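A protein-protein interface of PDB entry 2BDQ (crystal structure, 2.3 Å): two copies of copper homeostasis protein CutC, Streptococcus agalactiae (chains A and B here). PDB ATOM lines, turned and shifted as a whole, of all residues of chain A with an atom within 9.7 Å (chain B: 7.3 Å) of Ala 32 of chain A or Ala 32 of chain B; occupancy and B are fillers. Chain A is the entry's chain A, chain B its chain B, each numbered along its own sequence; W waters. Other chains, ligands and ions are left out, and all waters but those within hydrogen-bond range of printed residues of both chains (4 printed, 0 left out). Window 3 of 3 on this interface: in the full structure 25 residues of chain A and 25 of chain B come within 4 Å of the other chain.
Among the printed residues, merely in contact across the chains: Asp 29 of chain A with Asp 29 of chain B (3.7 Å) and Ala 32 of chain A with Ala 32 of chain B (3.8 Å).
Water W1 lies within hydrogen-bond range of the side-chain amide oxygen (OD1) of Asn 30 of chain A (2.7 Å), the side-chain carboxylate (OE1) of Glu 9 of chain B (3.1 Å), the backbone NH (N) of Ala 32 of chain B (3.3 Å) and the backbone NH (N) of Leu 31 of chain B (3.4 Å). Water W3 lies within hydrogen-bond range of OE2 of Glu 9 of chain B and N of Gly 65 of chain A. Water W4 lies within hydrogen-bond range of OD1 of Asn 30 of chain B, OE1 of Glu 9 of chain A, N of Ala 32 of chain A and N of Leu 31 of chain A. Water W2 bridges OD2 of Asp 29 of chain A and OD2 of Asp 29 of chain B.
OE2 of Glu 9 of chain A lies within hydrogen-bond range of ND2 of Asn 30 of chain B (3.0 Å). ND2 of Asn 30 of chain B lies within hydrogen-bond range of OD1 of Asp 29 of chain A, at 3.1 Å. The side-chain carboxylate (OD2) of Asp 29 of chain A lies within hydrogen-bond range of the side-chain hydroxyl (OG1) of Thr 36 of chain B (2.6 Å). ND2 of Asn 30 of chain A lies within hydrogen-bond range of OE2 of Glu 9 of chain B (3.0 Å). OD1 of Asp 29 of chain B lies within hydrogen-bond range of ND2 of Asn 30 of chain A, 2.9 Å away. The side-chain amide nitrogen (ND2) of Asn 30 of chain A lies close to the backbone NH (N) of Asn 30 of chain B, 3.3 Å away. The side-chain carboxylate (OD2) of Asp 29 of chain B sits at hydrogen-bond distance from the side-chain hydroxyl (OG1) of Thr 36 of chain A.
Of the 9 printed residues of chain B, 5 touch a printed residue of chain A. Hydrophobic or aromatic side chains of chain B that line the printed part of chain A: Ala 32. Among the printed residues, no Asp or Glu carboxylate lies within 4 Å of a Lys or Arg side-chain nitrogen of the other chain.
OE1 of Glu 9 of chain A lies within hydrogen-bond range of N of Leu 31 of chain A. The backbone NH of Gly 35 of chain A sits at hydrogen-bond distance from the backbone carbonyl oxygen of Asn 30 of chain A. The side-chain carboxylate (OE1) of Glu 9 of chain B is in hydrogen-bond range of the backbone NH (N) of Leu 31 of chain B (2.9 Å). The backbone carbonyl oxygen (O) of Asp 29 of chain B is in hydrogen-bond range of the backbone NH (N) of Thr 36 of chain B (2.8 Å). OD1 of Asn 30 of chain B sits close to N of Val 33 of chain B, at 3.4 Å. The backbone carbonyl oxygen (O) of Asn 30 of chain B sits at hydrogen-bond distance from the backbone NH (N) of Gly 35 of chain B (2.9 Å).
Printed residues of chain B within 4 Å of Asn 30 of chain A: Glu 9 (3.0 Å), Asp 29 (2.9 Å) and Asn 30 (3.3 Å). Of chain B, only Ala 32 comes within 4 Å of Ala 32 of chain A. Gly 66 of chain A touches none of the printed residues of chain B. Printed residues of chain A within 4 Å of Asp 29 of chain B: Asp 29, Asn 30 and Thr 36. Printed residues of chain A within 4 Å of Asn 30 of chain B: Glu 9, Asp 29 and Asn 30. Ala 32 of chain B touches just one residue of chain A: Ala 32 (3.8 Å). No residue of chain A comes within 4 Å of Val 33 of chain B. Of the printed residues of chain A, Thr 36 of chain B touches Asp 29. The nearest residue of chain B that does not touch Ala 32 of chain A is Asn 30 of chain B (5.0 Å). The nearest residue of chain A that does not touch Ala 32 of chain B is Asn 30 of chain A (5.2 Å).
Asp 29 of chain A touches its own counterpart, Asp 29 of chain B. Asp 29 of chain A touches Thr 36 of chain B, and with the chains exchanged Thr 36 of chain A touches Asp 29 of chain B. Asn 30 of chain A touches its own counterpart, Asn 30 of chain B. Ala 32 of chain A touches its own counterpart, Ala 32 of chain B. Of the 9 pairs that touch across the chains among the printed residues, 9 have their exchanged pair printed and touching as well.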
ATOM      1  N   CYS A   7      36.498  -6.519  10.300  1.00  0.00           N
ATOM      2  CA  CYS A   7      35.255  -6.070  10.921  1.00  0.00           C
ATOM      3  C   CYS A   7      34.625  -7.277  11.619  1.00  0.00           C
ATOM      4  O   CYS A   7      34.170  -8.216  10.965  1.00  0.00           O
ATOM      5  CB  CYS A   7      34.308  -5.519   9.844  1.00  0.00           C
ATOM      6  SG  CYS A   7      32.721  -4.855  10.455  1.00  0.00           S
ATOM      7  N   ALA A   8      34.597  -7.245  12.947  1.00  0.00           N
ATOM      8  CA  ALA A   8      34.065  -8.349  13.730  1.00  0.00           C
ATOM      9  C   ALA A   8      32.786  -8.034  14.485  1.00  0.00           C
ATOM     10  O   ALA A   8      32.461  -6.878  14.732  1.00  0.00           O
ATOM     11  CB  ALA A   8      35.137  -8.826  14.729  1.00  0.00           C
ATOM     12  N   GLU A   9      32.053  -9.081  14.829  1.00  0.00           N
ATOM     13  CA  GLU A   9      30.848  -8.936  15.629  1.00  0.00           C
ATOM     14  C   GLU A   9      31.208  -9.774  16.843  1.00  0.00           C
ATOM     15  O   GLU A   9      31.275 -11.007  16.753  1.00  0.00           O
ATOM     16  CB  GLU A   9      29.618  -9.519  14.926  1.00  0.00           C
ATOM     17  CG  GLU A   9      28.363  -9.455  15.794  1.00  0.00           C
ATOM     18  CD  GLU A   9      27.128  -9.998  15.108  1.00  0.00           C
ATOM     19  OE1 GLU A   9      26.717  -9.421  14.077  1.00  0.00           O
ATOM     20  OE2 GLU A   9      26.562 -11.001  15.601  1.00  0.00           O
ATOM     21  N   CYS A  28      32.484  -4.389  17.029  1.00  0.00           N
ATOM     22  CA  CYS A  28      31.107  -3.951  17.163  1.00  0.00           C
ATOM     23  C   CYS A  28      30.198  -5.161  17.290  1.00  0.00           C
ATOM     24  O   CYS A  28      30.668  -6.300  17.363  1.00  0.00           O
ATOM     25  CB  CYS A  28      30.679  -3.060  15.983  1.00  0.00           C
ATOM     26  SG  CYS A  28      31.287  -3.506  14.337  1.00  0.00           S
ATOM     27  N   ASP A  29      28.898  -4.920  17.368  1.00  0.00           N
ATOM     28  CA  ASP A  29      27.951  -6.012  17.455  1.00  0.00           C
ATOM     29  C   ASP A  29      26.882  -5.681  16.423  1.00  0.00           C
ATOM     30  O   ASP A  29      26.997  -4.681  15.708  1.00  0.00           O
ATOM     31  CB  ASP A  29      27.359  -6.088  18.871  1.00  0.00           C
ATOM     32  CG  ASP A  29      26.437  -7.281  19.061  1.00  0.00           C
ATOM     33  OD1 ASP A  29      26.633  -8.318  18.398  1.00  0.00           O
ATOM     34  OD2 ASP A  29      25.515  -7.197  19.890  1.00  0.00           O
ATOM     35  N   ASN A  30      25.871  -6.535  16.313  1.00  0.00           N
ATOM     36  CA  ASN A  30      24.767  -6.295  15.400  1.00  0.00           C
ATOM     37  C   ASN A  30      25.215  -5.870  13.994  1.00  0.00           C
ATOM     38  O   ASN A  30      24.833  -4.797  13.525  1.00  0.00           O
ATOM     39  CB  ASN A  30      23.883  -5.192  15.995  1.00  0.00           C
ATOM     40  CG  ASN A  30      22.463  -5.216  15.464  1.00  0.00           C
ATOM     41  OD1 ASN A  30      22.191  -5.761  14.398  1.00  0.00           O
ATOM     42  ND2 ASN A  30      21.549  -4.603  16.209  1.00  0.00           N
ATOM     43  N   LEU A  31      26.012  -6.690  13.314  1.00  0.00           N
ATOM     44  CA  LEU A  31      26.436  -6.317  11.966  1.00  0.00           C
ATOM     45  C   LEU A  31      25.278  -6.323  10.974  1.00  0.00           C
ATOM     46  O   LEU A  31      25.374  -5.743   9.889  1.00  0.00           O
ATOM     47  CB  LEU A  31      27.552  -7.239  11.477  1.00  0.00           C
ATOM     48  CG  LEU A  31      28.890  -6.990  12.185  1.00  0.00           C
ATOM     49  CD1 LEU A  31      29.967  -7.900  11.605  1.00  0.00           C
ATOM     50  CD2 LEU A  31      29.285  -5.536  12.020  1.00  0.00           C
ATOM     51  N   ALA A  32      24.175  -6.968  11.345  1.00  0.00           N
ATOM     52  CA  ALA A  32      23.014  -7.014  10.471  1.00  0.00           C
ATOM     53  C   ALA A  32      22.468  -5.611  10.224  1.00  0.00           C
ATOM     54  O   ALA A  32      21.848  -5.352   9.193  1.00  0.00           O
ATOM     55  CB  ALA A  32      21.930  -7.888  11.083  1.00  0.00           C
ATOM     56  N   VAL A  33      22.701  -4.701  11.163  1.00  0.00           N
ATOM     57  CA  VAL A  33      22.198  -3.344  11.013  1.00  0.00           C
ATOM     58  C   VAL A  33      23.347  -2.385  10.677  1.00  0.00           C
ATOM     59  O   VAL A  33      23.181  -1.163  10.654  1.00  0.00           O
ATOM     60  CB  VAL A  33      21.441  -2.903  12.303  1.00  0.00           C
ATOM     61  CG1 VAL A  33      22.422  -2.547  13.413  1.00  0.00           C
ATOM     62  CG2 VAL A  33      20.528  -1.749  11.991  1.00  0.00           C
ATOM     63  N   GLY A  34      24.515  -2.958  10.400  1.00  0.00           N
ATOM     64  CA  GLY A  34      25.672  -2.156  10.052  1.00  0.00           C
ATOM     65  C   GLY A  34      26.679  -2.009  11.177  1.00  0.00           C
ATOM     66  O   GLY A  34      27.738  -1.407  10.996  1.00  0.00           O
ATOM     67  N   GLY A  35      26.338  -2.538  12.349  1.00  0.00           N
ATOM     68  CA  GLY A  35      27.250  -2.468  13.478  1.00  0.00           C
ATOM     69  C   GLY A  35      26.899  -1.457  14.555  1.00  0.00           C
ATOM     70  O   GLY A  35      26.648  -0.289  14.261  1.00  0.00           O
ATOM     71  N   THR A  36      26.872  -1.904  15.803  1.00  0.00           N
ATOM     72  CA  THR A  36      26.582  -1.008  16.912  1.00  0.00           C
ATOM     73  C   THR A  36      27.639  -1.206  17.989  1.00  0.00           C
ATOM     74  O   THR A  36      28.534  -2.046  17.862  1.00  0.00           O
ATOM     75  CB  THR A  36      25.202  -1.280  17.550  1.00  0.00           C
ATOM     76  OG1 THR A  36      25.167  -2.609  18.080  1.00  0.00           O
ATOM     77  CG2 THR A  36      24.087  -1.106  16.532  1.00  0.00           C
ATOM     78  N   ARG A  62      27.972   3.573  18.137  1.00  0.00           N
ATOM     79  CA  ARG A  62      26.712   3.795  17.436  1.00  0.00           C
ATOM     80  C   ARG A  62      25.626   3.196  18.328  1.00  0.00           C
ATOM     81  O   ARG A  62      25.587   1.989  18.539  1.00  0.00           O
ATOM     82  CB  ARG A  62      26.756   3.097  16.078  1.00  0.00           C
ATOM     83  CG  ARG A  62      25.595   3.412  15.154  1.00  0.00           C
ATOM     84  CD  ARG A  62      25.845   2.752  13.809  1.00  0.00           C
ATOM     85  NE  ARG A  62      24.762   2.951  12.857  1.00  0.00           N
ATOM     86  CZ  ARG A  62      24.483   2.105  11.872  1.00  0.00           C
ATOM     87  NH1 ARG A  62      25.209   1.006  11.716  1.00  0.00           N
ATOM     88  NH2 ARG A  62      23.475   2.353  11.048  1.00  0.00           N
ATOM     89  N   ARG A  64      22.495   2.669  17.846  1.00  0.00           N
ATOM     90  CA  ARG A  64      21.511   1.845  17.159  1.00  0.00           C
ATOM     91  C   ARG A  64      21.699   1.912  15.650  1.00  0.00           C
ATOM     92  O   ARG A  64      22.579   2.619  15.151  1.00  0.00           O
ATOM     93  CB  ARG A  64      20.094   2.280  17.527  1.00  0.00           C
ATOM     94  CG  ARG A  64      19.859   3.774  17.447  1.00  0.00           C
ATOM     95  CD  ARG A  64      19.001   4.154  16.254  1.00  0.00           C
ATOM     96  NE  ARG A  64      18.734   5.591  16.226  1.00  0.00           N
ATOM     97  CZ  ARG A  64      18.903   6.355  15.147  1.00  0.00           C
ATOM     98  NH1 ARG A  64      19.330   5.813  14.011  1.00  0.00           N
ATOM     99  NH2 ARG A  64      18.676   7.663  15.200  1.00  0.00           N
ATOM    100  N   GLY A  65      20.876   1.168  14.927  1.00  0.00           N
ATOM    101  CA  GLY A  65      20.966   1.169  13.481  1.00  0.00           C
ATOM    102  C   GLY A  65      20.114   2.264  12.871  1.00  0.00           C
ATOM    103  O   GLY A  65      19.488   3.054  13.580  1.00  0.00           O
ATOM    104  N   GLY A  66      20.088   2.310  11.546  1.00  0.00           N
ATOM    105  CA  GLY A  66      19.312   3.325  10.865  1.00  0.00           C
ATOM    106  C   GLY A  66      20.124   4.594  10.701  1.00  0.00           C
ATOM    107  O   GLY A  66      21.339   4.534  10.512  1.00  0.00           O
ATOM    108  N   THR A 207      34.675  -7.660   6.313  1.00  0.00           N
ATOM    109  CA  THR A 207      34.391  -8.866   7.084  1.00  0.00           C
ATOM    110  C   THR A 207      35.091 -10.052   6.434  1.00  0.00           C
ATOM    111  O   THR A 207      35.386 -11.045   7.095  1.00  0.00           O
ATOM    112  CB  THR A 207      32.884  -9.175   7.149  1.00  0.00           C
ATOM    113  OG1 THR A 207      32.314  -9.103   5.834  1.00  0.00           O
ATOM    114  CG2 THR A 207      32.179  -8.202   8.073  1.00  0.00           C
ATOM    115  N   GLU B   9      15.207  -3.662  20.955  1.00  0.00           N
ATOM    116  CA  GLU B   9      16.589  -3.675  20.505  1.00  0.00           C
ATOM    117  C   GLU B   9      16.975  -2.221  20.724  1.00  0.00           C
ATOM    118  O   GLU B   9      16.512  -1.331  20.007  1.00  0.00           O
ATOM    119  CB  GLU B   9      16.716  -4.040  19.022  1.00  0.00           C
ATOM    120  CG  GLU B   9      18.156  -3.958  18.514  1.00  0.00           C
ATOM    121  CD  GLU B   9      18.307  -4.341  17.056  1.00  0.00           C
ATOM    122  OE1 GLU B   9      18.013  -5.509  16.707  1.00  0.00           O
ATOM    123  OE2 GLU B   9      18.720  -3.468  16.254  1.00  0.00           O
ATOM    124  N   ASP B  29      20.251  -6.247  22.211  1.00  0.00           N
ATOM    125  CA  ASP B  29      20.606  -5.675  20.923  1.00  0.00           C
ATOM    126  C   ASP B  29      20.654  -6.859  19.979  1.00  0.00           C
ATOM    127  O   ASP B  29      20.383  -7.989  20.397  1.00  0.00           O
ATOM    128  CB  ASP B  29      21.972  -4.979  21.009  1.00  0.00           C
ATOM    129  CG  ASP B  29      22.345  -4.249  19.728  1.00  0.00           C
ATOM    130  OD1 ASP B  29      21.447  -3.787  18.997  1.00  0.00           O
ATOM    131  OD2 ASP B  29      23.550  -4.112  19.456  1.00  0.00           O
ATOM    132  N   ASN B  30      20.966  -6.604  18.713  1.00  0.00           N
ATOM    133  CA  ASN B  30      21.096  -7.674  17.732  1.00  0.00           C
ATOM    134  C   ASN B  30      19.941  -8.678  17.767  1.00  0.00           C
ATOM    135  O   ASN B  30      20.167  -9.858  18.001  1.00  0.00           O
ATOM    136  CB  ASN B  30      22.416  -8.416  17.997  1.00  0.00           C
ATOM    137  CG  ASN B  30      22.942  -9.155  16.780  1.00  0.00           C
ATOM    138  OD1 ASN B  30      22.198  -9.463  15.853  1.00  0.00           O
ATOM    139  ND2 ASN B  30      24.236  -9.454  16.789  1.00  0.00           N
ATOM    140  N   LEU B  31      18.710  -8.229  17.547  1.00  0.00           N
ATOM    141  CA  LEU B  31      17.592  -9.169  17.559  1.00  0.00           C
ATOM    142  C   LEU B  31      17.635 -10.109  16.362  1.00  0.00           C
ATOM    143  O   LEU B  31      16.990 -11.155  16.353  1.00  0.00           O
ATOM    144  CB  LEU B  31      16.253  -8.428  17.602  1.00  0.00           C
ATOM    145  CG  LEU B  31      15.970  -7.778  18.965  1.00  0.00           C
ATOM    146  CD1 LEU B  31      14.596  -7.118  18.958  1.00  0.00           C
ATOM    147  CD2 LEU B  31      16.032  -8.839  20.061  1.00  0.00           C
ATOM    148  N   ALA B  32      18.409  -9.743  15.348  1.00  0.00           N
ATOM    149  CA  ALA B  32      18.521 -10.582  14.165  1.00  0.00           C
ATOM    150  C   ALA B  32      19.104 -11.950  14.529  1.00  0.00           C
ATOM    151  O   ALA B  32      18.825 -12.949  13.865  1.00  0.00           O
ATOM    152  CB  ALA B  32      19.400  -9.904  13.114  1.00  0.00           C
ATOM    153  N   VAL B  33      19.911 -11.994  15.584  1.00  0.00           N
ATOM    154  CA  VAL B  33      20.517 -13.253  15.997  1.00  0.00           C
ATOM    155  C   VAL B  33      19.828 -13.813  17.253  1.00  0.00           C
ATOM    156  O   VAL B  33      20.294 -14.781  17.860  1.00  0.00           O
ATOM    157  CB  VAL B  33      22.038 -13.061  16.229  1.00  0.00           C
ATOM    158  CG1 VAL B  33      22.301 -12.373  17.570  1.00  0.00           C
ATOM    159  CG2 VAL B  33      22.737 -14.384  16.160  1.00  0.00           C
ATOM    160  N   GLY B  34      18.708 -13.199  17.630  1.00  0.00           N
ATOM    161  CA  GLY B  34      17.967 -13.657  18.793  1.00  0.00           C
ATOM    162  C   GLY B  34      18.149 -12.774  20.009  1.00  0.00           C
ATOM    163  O   GLY B  34      17.493 -12.976  21.027  1.00  0.00           O
ATOM    164  N   GLY B  35      19.052 -11.800  19.910  1.00  0.00           N
ATOM    165  CA  GLY B  35      19.283 -10.888  21.016  1.00  0.00           C
ATOM    166  C   GLY B  35      20.570 -11.116  21.796  1.00  0.00           C
ATOM    167  O   GLY B  35      20.876 -12.236  22.211  1.00  0.00           O
ATOM    168  N   THR B  36      21.338 -10.052  21.995  1.00  0.00           N
ATOM    169  CA  THR B  36      22.569 -10.153  22.764  1.00  0.00           C
ATOM    170  C   THR B  36      22.598  -9.041  23.802  1.00  0.00           C
ATOM    171  O   THR B  36      21.680  -8.226  23.900  1.00  0.00           O
ATOM    172  CB  THR B  36      23.833 -10.012  21.888  1.00  0.00           C
ATOM    173  OG1 THR B  36      23.861  -8.712  21.293  1.00  0.00           O
ATOM    174  CG2 THR B  36      23.860 -11.065  20.800  1.00  0.00           C
HETATM  175  O   HOH W   1      19.784  -6.879  14.634  1.00  0.00           O
HETATM  176  O   HOH W   2      25.733  -4.815  21.955  1.00  0.00           O
HETATM  177  O   HOH W   3      19.134  -0.836  16.705  1.00  0.00           O
HETATM  178  O   HOH W   4      23.809  -9.089  13.441  1.00  0.00           O
